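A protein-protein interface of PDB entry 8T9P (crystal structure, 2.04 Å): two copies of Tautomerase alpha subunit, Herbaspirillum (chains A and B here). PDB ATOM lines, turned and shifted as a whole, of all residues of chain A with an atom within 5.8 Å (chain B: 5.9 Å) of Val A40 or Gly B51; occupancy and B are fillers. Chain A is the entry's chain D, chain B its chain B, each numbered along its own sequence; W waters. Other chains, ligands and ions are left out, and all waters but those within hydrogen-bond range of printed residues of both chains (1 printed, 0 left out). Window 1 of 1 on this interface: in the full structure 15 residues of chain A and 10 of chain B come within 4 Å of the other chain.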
ATOM      1  N   PRO A   1     -39.573  23.691   0.427  1.00  0.00           N
ATOM      2  CA  PRO A   1     -39.001  24.187  -0.835  1.00  0.00           C
ATOM      3  C   PRO A   1     -37.549  23.760  -0.983  1.00  0.00           C
ATOM      4  O   PRO A   1     -36.779  23.849  -0.015  1.00  0.00           O
ATOM      5  CB  PRO A   1     -39.119  25.710  -0.712  1.00  0.00           C
ATOM      6  CG  PRO A   1     -40.021  25.959   0.483  1.00  0.00           C
ATOM      7  CD  PRO A   1     -39.812  24.790   1.381  1.00  0.00           C
ATOM      8  N   ASN A   2     -37.194  23.266  -2.169  1.00  0.00           N
ATOM      9  CA  ASN A   2     -35.811  22.990  -2.533  1.00  0.00           C
ATOM     10  C   ASN A   2     -35.392  23.919  -3.660  1.00  0.00           C
ATOM     11  O   ASN A   2     -36.071  23.996  -4.691  1.00  0.00           O
ATOM     12  CB  ASN A   2     -35.652  21.535  -2.959  1.00  0.00           C
ATOM     13  CG  ASN A   2     -36.319  20.585  -1.962  1.00  0.00           C
ATOM     14  OD1 ASN A   2     -35.782  20.356  -0.880  1.00  0.00           O
ATOM     15  ND2 ASN A   2     -37.520  20.121  -2.284  1.00  0.00           N
ATOM     16  N   ILE A   3     -34.270  24.605  -3.472  1.00  0.00           N
ATOM     17  CA  ILE A   3     -33.754  25.551  -4.464  1.00  0.00           C
ATOM     18  C   ILE A   3     -32.361  25.085  -4.851  1.00  0.00           C
ATOM     19  O   ILE A   3     -31.451  25.045  -4.011  1.00  0.00           O
ATOM     20  CB  ILE A   3     -33.750  26.989  -3.935  1.00  0.00           C
ATOM     21  CG1 ILE A   3     -35.179  27.386  -3.587  1.00  0.00           C
ATOM     22  CG2 ILE A   3     -33.202  27.987  -4.987  1.00  0.00           C
ATOM     23  CD1 ILE A   3     -35.283  28.150  -2.358  1.00  0.00           C
ATOM     24  N   GLU A   4     -32.204  24.683  -6.108  1.00  0.00           N
ATOM     25  CA  GLU A   4     -30.900  24.412  -6.697  1.00  0.00           C
ATOM     26  C   GLU A   4     -30.560  25.532  -7.675  1.00  0.00           C
ATOM     27  O   GLU A   4     -31.323  25.790  -8.620  1.00  0.00           O
ATOM     28  CB  GLU A   4     -30.898  23.068  -7.408  1.00  0.00           C
ATOM     29  CG  GLU A   4     -29.554  22.669  -7.971  1.00  0.00           C
ATOM     30  CD  GLU A   4     -29.611  21.308  -8.629  1.00  0.00           C
ATOM     31  OE1 GLU A   4     -30.732  20.826  -8.913  1.00  0.00           O
ATOM     32  OE2 GLU A   4     -28.536  20.722  -8.865  1.00  0.00           O
ATOM     33  N   LEU A  19     -25.251  34.163  -1.218  1.00  0.00           N
ATOM     34  CA  LEU A  19     -26.260  33.700  -2.164  1.00  0.00           C
ATOM     35  C   LEU A  19     -27.223  32.713  -1.513  1.00  0.00           C
ATOM     36  O   LEU A  19     -28.446  32.841  -1.663  1.00  0.00           O
ATOM     37  CB  LEU A  19     -25.572  33.063  -3.370  1.00  0.00           C
ATOM     38  CG  LEU A  19     -26.357  32.768  -4.641  1.00  0.00           C
ATOM     39  CD1 LEU A  19     -26.997  34.031  -5.176  1.00  0.00           C
ATOM     40  CD2 LEU A  19     -25.366  32.193  -5.679  1.00  0.00           C
ATOM     41  N   VAL A  20     -26.704  31.708  -0.793  1.00  0.00           N
ATOM     42  CA  VAL A  20     -27.625  30.748  -0.183  1.00  0.00           C
ATOM     43  C   VAL A  20     -28.497  31.452   0.860  1.00  0.00           C
ATOM     44  O   VAL A  20     -29.685  31.137   1.009  1.00  0.00           O
ATOM     45  CB  VAL A  20     -26.889  29.527   0.420  1.00  0.00           C
ATOM     46  CG1 VAL A  20     -25.988  28.826  -0.593  1.00  0.00           C
ATOM     47  CG2 VAL A  20     -26.176  29.843   1.694  1.00  0.00           C
ATOM     48  N   LEU A  23     -31.091  33.668  -1.235  1.00  0.00           N
ATOM     49  CA  LEU A  23     -32.086  32.796  -1.845  1.00  0.00           C
ATOM     50  C   LEU A  23     -33.060  32.256  -0.804  1.00  0.00           C
ATOM     51  O   LEU A  23     -34.271  32.188  -1.051  1.00  0.00           O
ATOM     52  CB  LEU A  23     -31.401  31.642  -2.584  1.00  0.00           C
ATOM     53  CG  LEU A  23     -30.658  32.000  -3.880  1.00  0.00           C
ATOM     54  CD1 LEU A  23     -29.901  30.792  -4.423  1.00  0.00           C
ATOM     55  CD2 LEU A  23     -31.587  32.588  -4.948  1.00  0.00           C
ATOM     56  N   THR A  24     -32.545  31.862   0.361  1.00  0.00           N
ATOM     57  CA  THR A  24     -33.396  31.371   1.445  1.00  0.00           C
ATOM     58  C   THR A  24     -34.385  32.439   1.901  1.00  0.00           C
ATOM     59  O   THR A  24     -35.588  32.184   2.018  1.00  0.00           O
ATOM     60  CB  THR A  24     -32.521  30.928   2.626  1.00  0.00           C
ATOM     61  OG1 THR A  24     -31.590  29.934   2.184  1.00  0.00           O
ATOM     62  CG2 THR A  24     -33.380  30.330   3.764  1.00  0.00           C
ATOM     63  N   THR A  27     -37.221  33.188  -0.490  1.00  0.00           N
ATOM     64  CA  THR A  27     -38.270  32.179  -0.447  1.00  0.00           C
ATOM     65  C   THR A  27     -39.188  32.397   0.752  1.00  0.00           C
ATOM     66  O   THR A  27     -40.419  32.404   0.617  1.00  0.00           O
ATOM     67  CB  THR A  27     -37.629  30.797  -0.393  1.00  0.00           C
ATOM     68  OG1 THR A  27     -36.785  30.637  -1.538  1.00  0.00           O
ATOM     69  CG2 THR A  27     -38.692  29.672  -0.362  1.00  0.00           C
ATOM     70  N   VAL A  38     -36.543  25.418   4.277  1.00  0.00           N
ATOM     71  CA  VAL A  38     -35.979  25.778   2.976  1.00  0.00           C
ATOM     72  C   VAL A  38     -34.605  25.142   2.830  1.00  0.00           C
ATOM     73  O   VAL A  38     -33.718  25.338   3.671  1.00  0.00           O
ATOM     74  CB  VAL A  38     -35.892  27.308   2.821  1.00  0.00           C
ATOM     75  CG1 VAL A  38     -35.326  27.707   1.423  1.00  0.00           C
ATOM     76  CG2 VAL A  38     -37.253  27.940   3.076  1.00  0.00           C
ATOM     77  N   ARG A  39     -34.412  24.402   1.747  1.00  0.00           N
ATOM     78  CA  ARG A  39     -33.102  23.887   1.388  1.00  0.00           C
ATOM     79  C   ARG A  39     -32.642  24.586   0.120  1.00  0.00           C
ATOM     80  O   ARG A  39     -33.368  24.625  -0.878  1.00  0.00           O
ATOM     81  CB  ARG A  39     -33.134  22.370   1.206  1.00  0.00           C
ATOM     82  CG  ARG A  39     -33.366  21.666   2.532  1.00  0.00           C
ATOM     83  CD  ARG A  39     -33.251  20.165   2.453  1.00  0.00           C
ATOM     84  NE  ARG A  39     -34.109  19.554   3.468  1.00  0.00           N
ATOM     85  CZ  ARG A  39     -33.957  18.328   3.963  1.00  0.00           C
ATOM     86  NH1 ARG A  39     -32.951  17.561   3.559  1.00  0.00           N
ATOM     87  NH2 ARG A  39     -34.805  17.880   4.884  1.00  0.00           N
ATOM     88  N   VAL A  40     -31.450  25.158   0.175  1.00  0.00           N
ATOM     89  CA  VAL A  40     -30.846  25.846  -0.953  1.00  0.00           C
ATOM     90  C   VAL A  40     -29.471  25.246  -1.154  1.00  0.00           C
ATOM     91  O   VAL A  40     -28.687  25.165  -0.201  1.00  0.00           O
ATOM     92  CB  VAL A  40     -30.739  27.366  -0.712  1.00  0.00           C
ATOM     93  CG1 VAL A  40     -29.950  28.045  -1.846  1.00  0.00           C
ATOM     94  CG2 VAL A  40     -32.127  27.980  -0.559  1.00  0.00           C
ATOM     95  N   TRP A  41     -29.180  24.805  -2.374  1.00  0.00           N
ATOM     96  CA  TRP A  41     -27.811  24.423  -2.667  1.00  0.00           C
ATOM     97  C   TRP A  41     -27.395  24.959  -4.025  1.00  0.00           C
ATOM     98  O   TRP A  41     -28.223  25.227  -4.903  1.00  0.00           O
ATOM     99  CB  TRP A  41     -27.592  22.914  -2.590  1.00  0.00           C
ATOM    100  CG  TRP A  41     -28.334  22.099  -3.569  1.00  0.00           C
ATOM    101  CD1 TRP A  41     -27.831  21.521  -4.687  1.00  0.00           C
ATOM    102  CD2 TRP A  41     -29.714  21.711  -3.495  1.00  0.00           C
ATOM    103  NE1 TRP A  41     -28.814  20.808  -5.328  1.00  0.00           N
ATOM    104  CE2 TRP A  41     -29.983  20.922  -4.626  1.00  0.00           C
ATOM    105  CE3 TRP A  41     -30.752  21.975  -2.595  1.00  0.00           C
ATOM    106  CZ2 TRP A  41     -31.243  20.383  -4.879  1.00  0.00           C
ATOM    107  CZ3 TRP A  41     -32.000  21.443  -2.846  1.00  0.00           C
ATOM    108  CH2 TRP A  41     -32.238  20.657  -3.985  1.00  0.00           C
ATOM    109  N   LEU A  42     -26.098  25.147  -4.168  1.00  0.00           N
ATOM    110  CA  LEU A  42     -25.523  25.632  -5.405  1.00  0.00           C
ATOM    111  C   LEU A  42     -24.860  24.467  -6.106  1.00  0.00           C
ATOM    112  O   LEU A  42     -24.242  23.620  -5.461  1.00  0.00           O
ATOM    113  CB  LEU A  42     -24.502  26.742  -5.146  1.00  0.00           C
ATOM    114  CG  LEU A  42     -24.988  27.875  -4.242  1.00  0.00           C
ATOM    115  CD1 LEU A  42     -23.858  28.865  -4.007  1.00  0.00           C
ATOM    116  CD2 LEU A  42     -26.212  28.574  -4.841  1.00  0.00           C
ATOM    117  N   GLN B  49     -21.553  25.092  -0.225  1.00  0.00           N
ATOM    118  CA  GLN B  49     -22.568  25.318  -1.246  1.00  0.00           C
ATOM    119  C   GLN B  49     -23.934  24.742  -0.890  1.00  0.00           C
ATOM    120  O   GLN B  49     -24.833  24.759  -1.730  1.00  0.00           O
ATOM    121  CB  GLN B  49     -22.101  24.729  -2.582  1.00  0.00           C
ATOM    122  CG  GLN B  49     -20.868  25.397  -3.129  1.00  0.00           C
ATOM    123  CD  GLN B  49     -20.395  24.813  -4.444  1.00  0.00           C
ATOM    124  OE1 GLN B  49     -19.318  25.154  -4.912  1.00  0.00           O
ATOM    125  NE2 GLN B  49     -21.192  23.938  -5.045  1.00  0.00           N
ATOM    126  N   PHE B  50     -24.128  24.214   0.316  1.00  0.00           N
ATOM    127  CA  PHE B  50     -25.415  23.616   0.658  1.00  0.00           C
ATOM    128  C   PHE B  50     -25.895  24.192   1.981  1.00  0.00           C
ATOM    129  O   PHE B  50     -25.188  24.133   2.983  1.00  0.00           O
ATOM    130  CB  PHE B  50     -25.306  22.084   0.613  1.00  0.00           C
ATOM    131  CG  PHE B  50     -26.561  21.329   0.967  1.00  0.00           C
ATOM    132  CD1 PHE B  50     -27.794  21.943   0.988  1.00  0.00           C
ATOM    133  CD2 PHE B  50     -26.539  19.935   0.987  1.00  0.00           C
ATOM    134  CE1 PHE B  50     -28.955  21.225   1.251  1.00  0.00           C
ATOM    135  CE2 PHE B  50     -27.691  19.202   1.224  1.00  0.00           C
ATOM    136  CZ  PHE B  50     -28.897  19.844   1.352  1.00  0.00           C
ATOM    137  N   GLY B  51     -27.054  24.827   1.938  1.00  0.00           N
ATOM    138  CA  GLY B  51     -27.563  25.626   3.051  1.00  0.00           C
ATOM    139  C   GLY B  51     -28.751  25.003   3.691  1.00  0.00           C
ATOM    140  O   GLY B  51     -29.628  24.428   3.026  1.00  0.00           O
ATOM    141  N   ILE B  52     -28.815  25.072   5.021  1.00  0.00           N
ATOM    142  CA  ILE B  52     -29.949  24.623   5.808  1.00  0.00           C
ATOM    143  C   ILE B  52     -30.415  25.809   6.630  1.00  0.00           C
ATOM    144  O   ILE B  52     -29.621  26.397   7.371  1.00  0.00           O
ATOM    145  CB  ILE B  52     -29.591  23.432   6.711  1.00  0.00           C
ATOM    146  CG1 ILE B  52     -28.951  22.331   5.860  1.00  0.00           C
ATOM    147  CG2 ILE B  52     -30.830  22.926   7.456  1.00  0.00           C
ATOM    148  CD1 ILE B  52     -27.999  21.448   6.612  1.00  0.00           C
ATOM    149  N   GLY B  53     -31.687  26.178   6.475  1.00  0.00           N
ATOM    150  CA  GLY B  53     -32.197  27.361   7.131  1.00  0.00           C
ATOM    151  C   GLY B  53     -31.420  28.622   6.833  1.00  0.00           C
ATOM    152  O   GLY B  53     -31.405  29.537   7.659  1.00  0.00           O
ATOM    153  N   GLY B  54     -30.750  28.691   5.681  1.00  0.00           N
ATOM    154  CA  GLY B  54     -30.051  29.889   5.281  1.00  0.00           C
ATOM    155  C   GLY B  54     -28.573  29.928   5.600  1.00  0.00           C
ATOM    156  O   GLY B  54     -27.901  30.884   5.198  1.00  0.00           O
ATOM    157  N   LYS B  55     -28.047  28.938   6.314  1.00  0.00           N
ATOM    158  CA  LYS B  55     -26.631  28.884   6.654  1.00  0.00           C
ATOM    159  C   LYS B  55     -25.985  27.727   5.914  1.00  0.00           C
ATOM    160  O   LYS B  55     -26.602  26.669   5.759  1.00  0.00           O
ATOM    161  CB  LYS B  55     -26.422  28.697   8.165  1.00  0.00           C
ATOM    162  CG  LYS B  55     -27.023  29.784   9.045  1.00  0.00           C
ATOM    163  CD  LYS B  55     -26.681  29.560  10.531  1.00  0.00           C
ATOM    164  CE  LYS B  55     -25.376  28.777  10.704  1.00  0.00           C
ATOM    165  NZ  LYS B  55     -25.006  28.507  12.123  1.00  0.00           N
ATOM    166  N   THR B  56     -24.745  27.913   5.466  1.00  0.00           N
ATOM    167  CA  THR B  56     -24.050  26.807   4.820  1.00  0.00           C
ATOM    168  C   THR B  56     -23.659  25.748   5.849  1.00  0.00           C
ATOM    169  O   THR B  56     -23.474  26.037   7.037  1.00  0.00           O
ATOM    170  CB  THR B  56     -22.805  27.286   4.056  1.00  0.00           C
ATOM    171  OG1 THR B  56     -21.850  27.849   4.959  1.00  0.00           O
ATOM    172  CG2 THR B  56     -23.161  28.326   2.995  1.00  0.00           C
ATOM    173  N   VAL B  57     -23.560  24.502   5.381  1.00  0.00           N
ATOM    174  CA  VAL B  57     -23.083  23.421   6.236  1.00  0.00           C
ATOM    175  C   VAL B  57     -21.679  23.731   6.740  1.00  0.00           C
ATOM    176  O   VAL B  57     -21.342  23.448   7.896  1.00  0.00           O
ATOM    177  CB  VAL B  57     -23.140  22.081   5.478  1.00  0.00           C
ATOM    178  CG1 VAL B  57     -22.220  21.056   6.117  1.00  0.00           C
ATOM    179  CG2 VAL B  57     -24.576  21.564   5.423  1.00  0.00           C
HETATM  180  O   HOH W   1     -31.434  27.173   3.141  1.00  0.00           O
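The backbone carbonyl oxygen (O) of Val A40 sits at hydrogen-bond distance from the backbone NH (N) of Gly B51. The backbone carbonyl oxygen of Gln B49 is in hydrogen-bond range of the backbone NH of Leu A42, 2.8 Å away.
The backbone carbonyl oxygen (O) of Ile A3 lies within hydrogen-bond range of the backbone NH (N) of Trp A41 (2.8 Å). The backbone NH of Arg A39 lies within hydrogen-bond range of the backbone carbonyl oxygen of Pro A1, at 3.0 Å. The backbone NH of Val B57 lies within hydrogen-bond range of the backbone carbonyl oxygen of Phe B50 (2.9 Å). O of Val A20 sits at hydrogen-bond distance from OG1 of Thr A24, at 2.5 Å. The backbone carbonyl oxygen of Arg A39 sits at hydrogen-bond distance from the backbone NH of Ile A3, at 2.7 Å.
Among the printed residues, pairs that only touch across the chains: Trp A41 with Gln B49, Thr A24 with Gly B54, Val A40 with Phe B50, Val A38 with Gly B53, Val A20 with Thr B56, Trp A41 with Phe B50 and Arg A39 with Gly B51.
Of the printed residues of chain B, Val A40 touches Phe B50 (3.5 Å) and Gly B51 (2.7 Å). Gly B51 touches just these residues of chain A: Arg A39 and Val A40. Of the printed residues of chain B, Leu A42 touches Gln B49 (2.8 Å). Of the printed residues of chain A, Gly B53 touches Val A38. Printed residues of chain A within 4 Å of Thr B56: Val A20 (3.6 Å). Leu A23 touches none of the printed residues of chain B. Ile B52 touches none of the printed residues of chain A.
Of the 14 printed residues of chain A, 7 touch a printed residue of chain B. Hydrophobic or aromatic side chains of chain A that line the printed part of chain B: Val A20, Trp A41 and Leu A42. Hydrophobic or aromatic side chains of chain B that line the printed part of chain A: Phe B50. Among the printed residues, no Asp or Glu carboxylate lies within 4 Å of a Lys or Arg side-chain nitrogen of the other chain.
No position is printed for both chains.
Water W1 lies within hydrogen-bond range of the side-chain hydroxyl of Thr A24 (2.9 Å), the backbone carbonyl oxygen of Val A38 (3.0 Å), the backbone NH of Gly B54 (3.0 Å), the backbone carbonyl oxygen of Gly B51 (3.3 Å) and the backbone NH of Gly B53 (3.5 Å).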
